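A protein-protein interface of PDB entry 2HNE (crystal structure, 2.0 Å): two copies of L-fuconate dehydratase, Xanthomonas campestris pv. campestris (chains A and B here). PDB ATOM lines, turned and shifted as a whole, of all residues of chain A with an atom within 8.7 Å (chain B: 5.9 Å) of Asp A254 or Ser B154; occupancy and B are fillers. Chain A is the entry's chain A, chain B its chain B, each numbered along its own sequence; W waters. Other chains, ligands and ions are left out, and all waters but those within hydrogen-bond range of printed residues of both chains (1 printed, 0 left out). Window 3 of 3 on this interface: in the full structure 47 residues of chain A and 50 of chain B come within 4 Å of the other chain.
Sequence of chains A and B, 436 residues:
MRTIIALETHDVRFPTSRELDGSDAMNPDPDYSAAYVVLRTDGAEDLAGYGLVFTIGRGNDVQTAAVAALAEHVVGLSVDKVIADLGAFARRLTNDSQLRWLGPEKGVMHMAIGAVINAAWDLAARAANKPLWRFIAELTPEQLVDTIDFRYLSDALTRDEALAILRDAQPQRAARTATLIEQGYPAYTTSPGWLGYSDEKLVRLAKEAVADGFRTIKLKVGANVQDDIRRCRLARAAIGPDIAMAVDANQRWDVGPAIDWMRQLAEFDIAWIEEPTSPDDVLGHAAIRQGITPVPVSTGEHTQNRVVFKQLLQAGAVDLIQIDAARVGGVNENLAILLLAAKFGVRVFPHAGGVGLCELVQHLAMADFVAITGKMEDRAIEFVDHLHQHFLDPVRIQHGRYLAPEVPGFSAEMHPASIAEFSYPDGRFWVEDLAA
N of Tyr B152 sits at hydrogen-bond distance from OD2 of Asp A254, 2.8 Å away. The side-chain hydroxyl of Tyr B152 sits at hydrogen-bond distance from the backbone carbonyl oxygen of Gln A251 (2.5 Å). The side-chain carboxylate (OD1) of Asp A254 sits at hydrogen-bond distance from the side-chain hydroxyl (OG) of Ser B154 (2.8 Å).
The backbone carbonyl oxygen (O) of Ser A278 lies within hydrogen-bond range of a ring nitrogen (NE2) of His A285, 3.1 Å away. The backbone NH of Gln A251 sits at hydrogen-bond distance from the backbone carbonyl oxygen of Glu A275 (2.7 Å). OG1 of Thr A277 lies within hydrogen-bond range of O of Trp A253, at 2.7 Å. O of Pro A276 lies within hydrogen-bond range of N of Trp A253, 3.2 Å away.
Among the printed residues, merely in contact across the chains: Thr A277 with Tyr B152 (3.5 Å), Ser A278 with Tyr B152 (3.5 Å), Trp A253 with Tyr B152 (3.7 Å), Asp A254 with Arg B151 (3.8 Å), Asp A254 with Leu B153 (3.9 Å), Asp A254 with Phe B150 (3.9 Å) and Val A255 with Asp B155 (3.99 Å).
Of the printed residues of chain B, Gln A251 touches Tyr B152. Asp A254 touches just these residues of chain B: Phe B150, Arg B151, Tyr B152, Leu B153 and Ser B154. Gly A256 touches none of the printed residues of chain B. Pro A276 touches none of the printed residues of chain B. Printed residues of chain A within 4 Å of Leu B153: Asp A254. Of chain A, only Asp A254 (2.8 Å) comes within 4 Å of Ser B154. The nearest residue of chain A that does not touch Ser B154 is Pro A257 (4.7 Å).
Along chain A the printed residues that touch a printed residue of chain B span positions 251 to 278. Of the 10 printed residues of chain B, 6 touch a printed residue of chain A. Hydrophobic or aromatic side chains of chain B that line the printed part of chain A: Tyr B152.
No position is printed for both chains. Of the 10 pairs that touch across the chains among the printed residues, none has its exchanged pair printed and touching as well.
Water W1 lies within hydrogen-bond range of the backbone NH (N) of Gly A256 (2.8 Å) and the side-chain hydroxyl (OG) of Ser B154 (3.0 Å).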
ATOM      1  N   ALA A 249     -27.418   1.750  -2.587  1.00  0.00           N
ATOM      2  CA  ALA A 249     -26.941   2.930  -3.314  1.00  0.00           C
ATOM      3  C   ALA A 249     -25.635   3.473  -2.734  1.00  0.00           C
ATOM      4  O   ALA A 249     -25.027   4.394  -3.282  1.00  0.00           O
ATOM      5  CB  ALA A 249     -28.006   4.013  -3.307  1.00  0.00           C
ATOM      6  N   GLN A 251     -24.785   5.484  -0.262  1.00  0.00           N
ATOM      7  CA  GLN A 251     -24.704   6.917   0.052  1.00  0.00           C
ATOM      8  C   GLN A 251     -24.575   7.896  -1.119  1.00  0.00           C
ATOM      9  O   GLN A 251     -24.308   9.078  -0.910  1.00  0.00           O
ATOM     10  CB  GLN A 251     -23.516   7.142   0.999  1.00  0.00           C
ATOM     11  CG  GLN A 251     -23.430   6.180   2.203  1.00  0.00           C
ATOM     12  CD  GLN A 251     -22.086   6.283   2.948  1.00  0.00           C
ATOM     13  OE1 GLN A 251     -21.251   7.125   2.622  1.00  0.00           O
ATOM     14  NE2 GLN A 251     -21.882   5.425   3.949  1.00  0.00           N
ATOM     15  N   ARG A 252     -24.782   7.427  -2.344  1.00  0.00           N
ATOM     16  CA  ARG A 252     -24.604   8.281  -3.517  1.00  0.00           C
ATOM     17  C   ARG A 252     -25.537   9.458  -3.755  1.00  0.00           C
ATOM     18  O   ARG A 252     -25.096  10.511  -4.202  1.00  0.00           O
ATOM     19  CB  ARG A 252     -24.604   7.414  -4.787  1.00  0.00           C
ATOM     20  CG  ARG A 252     -23.546   6.314  -4.784  1.00  0.00           C
ATOM     21  CD  ARG A 252     -23.677   5.393  -5.997  1.00  0.00           C
ATOM     22  NE  ARG A 252     -23.408   6.100  -7.244  1.00  0.00           N
ATOM     23  CZ  ARG A 252     -22.447   5.765  -8.102  1.00  0.00           C
ATOM     24  NH1 ARG A 252     -21.659   4.726  -7.851  1.00  0.00           N
ATOM     25  NH2 ARG A 252     -22.269   6.480  -9.207  1.00  0.00           N
ATOM     26  N   TRP A 253     -26.815   9.304  -3.441  1.00  0.00           N
ATOM     27  CA  TRP A 253     -27.775  10.347  -3.767  1.00  0.00           C
ATOM     28  C   TRP A 253     -28.115  11.422  -2.755  1.00  0.00           C
ATOM     29  O   TRP A 253     -27.890  11.257  -1.561  1.00  0.00           O
ATOM     30  CB  TRP A 253     -29.100   9.706  -4.176  1.00  0.00           C
ATOM     31  CG  TRP A 253     -28.991   8.545  -5.127  1.00  0.00           C
ATOM     32  CD1 TRP A 253     -28.310   8.509  -6.315  1.00  0.00           C
ATOM     33  CD2 TRP A 253     -29.682   7.290  -5.022  1.00  0.00           C
ATOM     34  NE1 TRP A 253     -28.544   7.306  -6.960  1.00  0.00           N
ATOM     35  CE2 TRP A 253     -29.382   6.545  -6.188  1.00  0.00           C
ATOM     36  CE3 TRP A 253     -30.531   6.727  -4.059  1.00  0.00           C
ATOM     37  CZ2 TRP A 253     -29.905   5.270  -6.415  1.00  0.00           C
ATOM     38  CZ3 TRP A 253     -31.053   5.455  -4.284  1.00  0.00           C
ATOM     39  CH2 TRP A 253     -30.734   4.741  -5.459  1.00  0.00           C
ATOM     40  N   ASP A 254     -28.660  12.519  -3.281  1.00  0.00           N
ATOM     41  CA  ASP A 254     -29.181  13.605  -2.462  1.00  0.00           C
ATOM     42  C   ASP A 254     -30.640  13.170  -2.338  1.00  0.00           C
ATOM     43  O   ASP A 254     -31.079  12.248  -3.042  1.00  0.00           O
ATOM     44  CB  ASP A 254     -29.114  14.950  -3.183  1.00  0.00           C
ATOM     45  CG  ASP A 254     -27.780  15.648  -3.006  1.00  0.00           C
ATOM     46  OD1 ASP A 254     -27.730  16.882  -3.191  1.00  0.00           O
ATOM     47  OD2 ASP A 254     -26.776  14.977  -2.684  1.00  0.00           O
ATOM     48  N   VAL A 255     -31.397  13.825  -1.469  1.00  0.00           N
ATOM     49  CA  VAL A 255     -32.791  13.464  -1.243  1.00  0.00           C
ATOM     50  C   VAL A 255     -33.705  13.425  -2.472  1.00  0.00           C
ATOM     51  O   VAL A 255     -34.327  12.392  -2.762  1.00  0.00           O
ATOM     52  CB  VAL A 255     -33.405  14.396  -0.172  1.00  0.00           C
ATOM     53  CG1 VAL A 255     -34.898  14.115  -0.008  1.00  0.00           C
ATOM     54  CG2 VAL A 255     -32.666  14.182   1.143  1.00  0.00           C
ATOM     55  N   GLY A 256     -33.808  14.542  -3.181  1.00  0.00           N
ATOM     56  CA  GLY A 256     -34.660  14.568  -4.353  1.00  0.00           C
ATOM     57  C   GLY A 256     -34.313  13.468  -5.347  1.00  0.00           C
ATOM     58  O   GLY A 256     -35.167  12.665  -5.718  1.00  0.00           O
ATOM     59  N   PRO A 257     -33.059  13.403  -5.796  1.00  0.00           N
ATOM     60  CA  PRO A 257     -32.667  12.368  -6.760  1.00  0.00           C
ATOM     61  C   PRO A 257     -32.998  10.943  -6.330  1.00  0.00           C
ATOM     62  O   PRO A 257     -33.432  10.130  -7.146  1.00  0.00           O
ATOM     63  CB  PRO A 257     -31.171  12.614  -6.925  1.00  0.00           C
ATOM     64  CG  PRO A 257     -31.108  14.122  -6.851  1.00  0.00           C
ATOM     65  CD  PRO A 257     -32.005  14.425  -5.664  1.00  0.00           C
ATOM     66  N   ALA A 258     -32.800  10.655  -5.047  1.00  0.00           N
ATOM     67  CA  ALA A 258     -33.065   9.335  -4.493  1.00  0.00           C
ATOM     68  C   ALA A 258     -34.519   8.948  -4.676  1.00  0.00           C
ATOM     69  O   ALA A 258     -34.830   7.805  -5.036  1.00  0.00           O
ATOM     70  CB  ALA A 258     -32.707   9.311  -3.006  1.00  0.00           C
ATOM     71  N   ILE A 259     -35.410   9.894  -4.407  1.00  0.00           N
ATOM     72  CA  ILE A 259     -36.833   9.641  -4.538  1.00  0.00           C
ATOM     73  C   ILE A 259     -37.207   9.393  -5.994  1.00  0.00           C
ATOM     74  O   ILE A 259     -37.942   8.451  -6.291  1.00  0.00           O
ATOM     75  CB  ILE A 259     -37.668  10.812  -3.990  1.00  0.00           C
ATOM     76  CG1 ILE A 259     -37.460  10.931  -2.475  1.00  0.00           C
ATOM     77  CG2 ILE A 259     -39.129  10.582  -4.289  1.00  0.00           C
ATOM     78  CD1 ILE A 259     -38.092  12.163  -1.874  1.00  0.00           C
ATOM     79  N   ASP A 260     -36.699  10.233  -6.890  1.00  0.00           N
ATOM     80  CA  ASP A 260     -36.980  10.082  -8.315  1.00  0.00           C
ATOM     81  C   ASP A 260     -36.459   8.744  -8.826  1.00  0.00           C
ATOM     82  O   ASP A 260     -37.124   8.056  -9.605  1.00  0.00           O
ATOM     83  CB  ASP A 260     -36.326  11.219  -9.107  1.00  0.00           C
ATOM     84  CG  ASP A 260     -37.068  12.548  -8.956  1.00  0.00           C
ATOM     85  OD1 ASP A 260     -36.493  13.591  -9.324  1.00  0.00           O
ATOM     86  OD2 ASP A 260     -38.228  12.552  -8.483  1.00  0.00           O
ATOM     87  N   TRP A 261     -35.263   8.387  -8.369  1.00  0.00           N
ATOM     88  CA  TRP A 261     -34.599   7.156  -8.764  1.00  0.00           C
ATOM     89  C   TRP A 261     -35.333   5.900  -8.298  1.00  0.00           C
ATOM     90  O   TRP A 261     -35.689   5.039  -9.115  1.00  0.00           O
ATOM     91  CB  TRP A 261     -33.179   7.157  -8.208  1.00  0.00           C
ATOM     92  CG  TRP A 261     -32.236   6.221  -8.890  1.00  0.00           C
ATOM     93  CD1 TRP A 261     -32.294   4.855  -8.909  1.00  0.00           C
ATOM     94  CD2 TRP A 261     -31.036   6.582  -9.588  1.00  0.00           C
ATOM     95  NE1 TRP A 261     -31.195   4.343  -9.566  1.00  0.00           N
ATOM     96  CE2 TRP A 261     -30.409   5.382  -9.993  1.00  0.00           C
ATOM     97  CE3 TRP A 261     -30.430   7.803  -9.905  1.00  0.00           C
ATOM     98  CZ2 TRP A 261     -29.198   5.370 -10.700  1.00  0.00           C
ATOM     99  CZ3 TRP A 261     -29.226   7.791 -10.606  1.00  0.00           C
ATOM    100  CH2 TRP A 261     -28.625   6.578 -10.994  1.00  0.00           C
ATOM    101  N   GLU A 275     -28.732   2.626   2.389  1.00  0.00           N
ATOM    102  CA  GLU A 275     -27.971   3.866   2.318  1.00  0.00           C
ATOM    103  C   GLU A 275     -28.254   4.754   1.118  1.00  0.00           C
ATOM    104  O   GLU A 275     -27.345   5.058   0.346  1.00  0.00           O
ATOM    105  CB  GLU A 275     -26.474   3.580   2.360  1.00  0.00           C
ATOM    106  CG  GLU A 275     -26.008   2.890   3.612  1.00  0.00           C
ATOM    107  CD  GLU A 275     -24.580   3.257   3.952  1.00  0.00           C
ATOM    108  OE1 GLU A 275     -24.373   4.249   4.690  1.00  0.00           O
ATOM    109  OE2 GLU A 275     -23.663   2.565   3.462  1.00  0.00           O
ATOM    110  N   PRO A 276     -29.507   5.196   0.940  1.00  0.00           N
ATOM    111  CA  PRO A 276     -29.754   6.057  -0.220  1.00  0.00           C
ATOM    112  C   PRO A 276     -28.928   7.339  -0.172  1.00  0.00           C
ATOM    113  O   PRO A 276     -28.488   7.835  -1.198  1.00  0.00           O
ATOM    114  CB  PRO A 276     -31.255   6.324  -0.144  1.00  0.00           C
ATOM    115  CG  PRO A 276     -31.554   6.192   1.330  1.00  0.00           C
ATOM    116  CD  PRO A 276     -30.751   4.968   1.691  1.00  0.00           C
ATOM    117  N   THR A 277     -28.686   7.869   1.021  1.00  0.00           N
ATOM    118  CA  THR A 277     -27.918   9.108   1.096  1.00  0.00           C
ATOM    119  C   THR A 277     -26.856   9.113   2.201  1.00  0.00           C
ATOM    120  O   THR A 277     -26.481   8.061   2.717  1.00  0.00           O
ATOM    121  CB  THR A 277     -28.893  10.301   1.254  1.00  0.00           C
ATOM    122  OG1 THR A 277     -28.189  11.541   1.089  1.00  0.00           O
ATOM    123  CG2 THR A 277     -29.588  10.257   2.630  1.00  0.00           C
ATOM    124  N   SER A 278     -26.352  10.299   2.539  1.00  0.00           N
ATOM    125  CA  SER A 278     -25.347  10.438   3.596  1.00  0.00           C
ATOM    126  C   SER A 278     -25.769   9.714   4.878  1.00  0.00           C
ATOM    127  O   SER A 278     -26.921   9.800   5.295  1.00  0.00           O
ATOM    128  CB  SER A 278     -25.126  11.923   3.912  1.00  0.00           C
ATOM    129  OG  SER A 278     -24.438  12.070   5.139  1.00  0.00           O
ATOM    130  N   ASP A 281     -27.383  11.937   7.523  1.00  0.00           N
ATOM    131  CA  ASP A 281     -28.645  12.592   7.240  1.00  0.00           C
ATOM    132  C   ASP A 281     -29.891  11.848   7.714  1.00  0.00           C
ATOM    133  O   ASP A 281     -30.585  11.175   6.939  1.00  0.00           O
ATOM    134  CB  ASP A 281     -28.750  12.894   5.746  1.00  0.00           C
ATOM    135  CG  ASP A 281     -29.637  14.090   5.460  1.00  0.00           C
ATOM    136  OD1 ASP A 281     -29.609  14.574   4.311  1.00  0.00           O
ATOM    137  OD2 ASP A 281     -30.355  14.549   6.380  1.00  0.00           O
ATOM    138  N   GLY A 284     -32.994  13.324   6.104  1.00  0.00           N
ATOM    139  CA  GLY A 284     -33.058  13.014   4.681  1.00  0.00           C
ATOM    140  C   GLY A 284     -33.576  11.608   4.399  1.00  0.00           C
ATOM    141  O   GLY A 284     -34.335  11.390   3.448  1.00  0.00           O
ATOM    142  N   HIS A 285     -33.164  10.653   5.222  1.00  0.00           N
ATOM    143  CA  HIS A 285     -33.599   9.277   5.058  1.00  0.00           C
ATOM    144  C   HIS A 285     -35.094   9.198   5.318  1.00  0.00           C
ATOM    145  O   HIS A 285     -35.799   8.421   4.690  1.00  0.00           O
ATOM    146  CB  HIS A 285     -32.845   8.351   6.018  1.00  0.00           C
ATOM    147  CG  HIS A 285     -31.459   8.003   5.566  1.00  0.00           C
ATOM    148  ND1 HIS A 285     -31.184   6.902   4.777  1.00  0.00           N
ATOM    149  CD2 HIS A 285     -30.266   8.591   5.814  1.00  0.00           C
ATOM    150  CE1 HIS A 285     -29.882   6.827   4.566  1.00  0.00           C
ATOM    151  NE2 HIS A 285     -29.303   7.839   5.186  1.00  0.00           N
ATOM    152  N   ALA A 287     -37.185  11.649   4.767  1.00  0.00           N
ATOM    153  CA  ALA A 287     -37.794  12.287   3.608  1.00  0.00           C
ATOM    154  C   ALA A 287     -37.881  11.320   2.424  1.00  0.00           C
ATOM    155  O   ALA A 287     -38.912  11.230   1.754  1.00  0.00           O
ATOM    156  CB  ALA A 287     -36.991  13.518   3.210  1.00  0.00           C
ATOM    157  N   ILE A 288     -36.786  10.613   2.175  1.00  0.00           N
ATOM    158  CA  ILE A 288     -36.731   9.635   1.088  1.00  0.00           C
ATOM    159  C   ILE A 288     -37.749   8.516   1.323  1.00  0.00           C
ATOM    160  O   ILE A 288     -38.544   8.187   0.437  1.00  0.00           O
ATOM    161  CB  ILE A 288     -35.310   9.054   0.984  1.00  0.00           C
ATOM    162  CG1 ILE A 288     -34.352  10.165   0.547  1.00  0.00           C
ATOM    163  CG2 ILE A 288     -35.291   7.844   0.018  1.00  0.00           C
ATOM    164  CD1 ILE A 288     -32.874   9.813   0.695  1.00  0.00           C
ATOM    165  N   PHE B 150     -21.710  21.050  -2.699  1.00  0.00           N
ATOM    166  CA  PHE B 150     -23.164  21.097  -2.575  1.00  0.00           C
ATOM    167  C   PHE B 150     -23.855  19.743  -2.434  1.00  0.00           C
ATOM    168  O   PHE B 150     -25.083  19.663  -2.359  1.00  0.00           O
ATOM    169  CB  PHE B 150     -23.779  21.857  -3.753  1.00  0.00           C
ATOM    170  CG  PHE B 150     -23.504  23.327  -3.725  1.00  0.00           C
ATOM    171  CD1 PHE B 150     -22.371  23.849  -4.339  1.00  0.00           C
ATOM    172  CD2 PHE B 150     -24.361  24.188  -3.046  1.00  0.00           C
ATOM    173  CE1 PHE B 150     -22.094  25.208  -4.277  1.00  0.00           C
ATOM    174  CE2 PHE B 150     -24.097  25.552  -2.974  1.00  0.00           C
ATOM    175  CZ  PHE B 150     -22.959  26.065  -3.592  1.00  0.00           C
ATOM    176  N   ARG B 151     -23.067  18.680  -2.402  1.00  0.00           N
ATOM    177  CA  ARG B 151     -23.603  17.330  -2.265  1.00  0.00           C
ATOM    178  C   ARG B 151     -24.247  17.187  -0.871  1.00  0.00           C
ATOM    179  O   ARG B 151     -23.671  17.616   0.125  1.00  0.00           O
ATOM    180  CB  ARG B 151     -22.453  16.348  -2.431  1.00  0.00           C
ATOM    181  CG  ARG B 151     -22.796  14.893  -2.311  1.00  0.00           C
ATOM    182  CD  ARG B 151     -21.543  14.228  -1.795  1.00  0.00           C
ATOM    183  NE  ARG B 151     -21.351  12.878  -2.283  1.00  0.00           N
ATOM    184  CZ  ARG B 151     -20.242  12.180  -2.076  1.00  0.00           C
ATOM    185  NH1 ARG B 151     -19.233  12.719  -1.390  1.00  0.00           N
ATOM    186  NH2 ARG B 151     -20.147  10.948  -2.555  1.00  0.00           N
ATOM    187  N   TYR B 152     -25.439  16.592  -0.828  1.00  0.00           N
ATOM    188  CA  TYR B 152     -26.220  16.386   0.394  1.00  0.00           C
ATOM    189  C   TYR B 152     -26.877  17.675   0.899  1.00  0.00           C
ATOM    190  O   TYR B 152     -27.435  17.694   1.999  1.00  0.00           O
ATOM    191  CB  TYR B 152     -25.368  15.780   1.516  1.00  0.00           C
ATOM    192  CG  TYR B 152     -24.694  14.475   1.152  1.00  0.00           C
ATOM    193  CD1 TYR B 152     -25.378  13.485   0.443  1.00  0.00           C
ATOM    194  CD2 TYR B 152     -23.377  14.226   1.523  1.00  0.00           C
ATOM    195  CE1 TYR B 152     -24.762  12.279   0.109  1.00  0.00           C
ATOM    196  CE2 TYR B 152     -22.749  13.023   1.196  1.00  0.00           C
ATOM    197  CZ  TYR B 152     -23.449  12.052   0.487  1.00  0.00           C
ATOM    198  OH  TYR B 152     -22.835  10.859   0.163  1.00  0.00           O
ATOM    199  N   LEU B 153     -26.829  18.736   0.091  1.00  0.00           N
ATOM    200  CA  LEU B 153     -27.412  20.028   0.466  1.00  0.00           C
ATOM    201  C   LEU B 153     -28.504  20.546  -0.467  1.00  0.00           C
ATOM    202  O   LEU B 153     -29.205  21.505  -0.135  1.00  0.00           O
ATOM    203  CB  LEU B 153     -26.318  21.100   0.538  1.00  0.00           C
ATOM    204  CG  LEU B 153     -25.238  20.910   1.595  1.00  0.00           C
ATOM    205  CD1 LEU B 153     -24.239  22.054   1.523  1.00  0.00           C
ATOM    206  CD2 LEU B 153     -25.897  20.849   2.971  1.00  0.00           C
ATOM    207  N   SER B 154     -28.671  19.915  -1.624  1.00  0.00           N
ATOM    208  CA  SER B 154     -29.651  20.411  -2.577  1.00  0.00           C
ATOM    209  C   SER B 154     -31.069  20.583  -2.034  1.00  0.00           C
ATOM    210  O   SER B 154     -31.870  21.299  -2.618  1.00  0.00           O
ATOM    211  CB  SER B 154     -29.657  19.535  -3.846  1.00  0.00           C
ATOM    212  OG  SER B 154     -30.118  18.221  -3.582  1.00  0.00           O
ATOM    213  N   ASP B 155     -31.396  19.952  -0.915  1.00  0.00           N
ATOM    214  CA  ASP B 155     -32.747  20.114  -0.372  1.00  0.00           C
ATOM    215  C   ASP B 155     -32.861  21.304   0.585  1.00  0.00           C
ATOM    216  O   ASP B 155     -33.941  21.576   1.119  1.00  0.00           O
ATOM    217  CB  ASP B 155     -33.198  18.838   0.343  1.00  0.00           C
ATOM    218  CG  ASP B 155     -32.185  18.341   1.361  1.00  0.00           C
ATOM    219  OD1 ASP B 155     -32.622  17.943   2.465  1.00  0.00           O
ATOM    220  OD2 ASP B 155     -30.963  18.328   1.057  1.00  0.00           O
ATOM    221  N   ALA B 156     -31.753  22.006   0.797  1.00  0.00           N
ATOM    222  CA  ALA B 156     -31.732  23.154   1.701  1.00  0.00           C
ATOM    223  C   ALA B 156     -30.991  24.337   1.099  1.00  0.00           C
ATOM    224  O   ALA B 156     -31.390  25.484   1.281  1.00  0.00           O
ATOM    225  CB  ALA B 156     -31.097  22.763   3.030  1.00  0.00           C
ATOM    226  N   LEU B 157     -29.900  24.059   0.399  1.00  0.00           N
ATOM    227  CA  LEU B 157     -29.118  25.111  -0.242  1.00  0.00           C
ATOM    228  C   LEU B 157     -28.599  24.642  -1.594  1.00  0.00           C
ATOM    229  O   LEU B 157     -27.659  23.850  -1.658  1.00  0.00           O
ATOM    230  CB  LEU B 157     -27.923  25.521   0.625  1.00  0.00           C
ATOM    231  CG  LEU B 157     -27.071  26.611  -0.030  1.00  0.00           C
ATOM    232  CD1 LEU B 157     -27.807  27.932   0.074  1.00  0.00           C
ATOM    233  CD2 LEU B 157     -25.715  26.711   0.627  1.00  0.00           C
ATOM    234  N   THR B 158     -29.214  25.129  -2.669  1.00  0.00           N
ATOM    235  CA  THR B 158     -28.780  24.766  -4.016  1.00  0.00           C
ATOM    236  C   THR B 158     -27.693  25.749  -4.430  1.00  0.00           C
ATOM    237  O   THR B 158     -27.516  26.790  -3.794  1.00  0.00           O
ATOM    238  CB  THR B 158     -29.937  24.852  -5.043  1.00  0.00           C
ATOM    239  OG1 THR B 158     -30.360  26.212  -5.175  1.00  0.00           O
ATOM    240  CG2 THR B 158     -31.118  24.002  -4.596  1.00  0.00           C
ATOM    241  N   GLU B 161     -29.108  29.084  -5.273  1.00  0.00           N
ATOM    242  CA  GLU B 161     -29.634  29.746  -4.085  1.00  0.00           C
ATOM    243  C   GLU B 161     -28.492  30.439  -3.354  1.00  0.00           C
ATOM    244  O   GLU B 161     -28.682  31.484  -2.724  1.00  0.00           O
ATOM    245  CB  GLU B 161     -30.318  28.733  -3.162  1.00  0.00           C
ATOM    246  CG  GLU B 161     -31.761  28.431  -3.550  1.00  0.00           C
ATOM    247  CD  GLU B 161     -32.371  27.293  -2.746  1.00  0.00           C
ATOM    248  OE1 GLU B 161     -33.611  27.140  -2.794  1.00  0.00           O
ATOM    249  OE2 GLU B 161     -31.615  26.549  -2.076  1.00  0.00           O
HETATM  250  O   HOH W   1     -32.703  17.042  -2.743  1.00  0.00           O
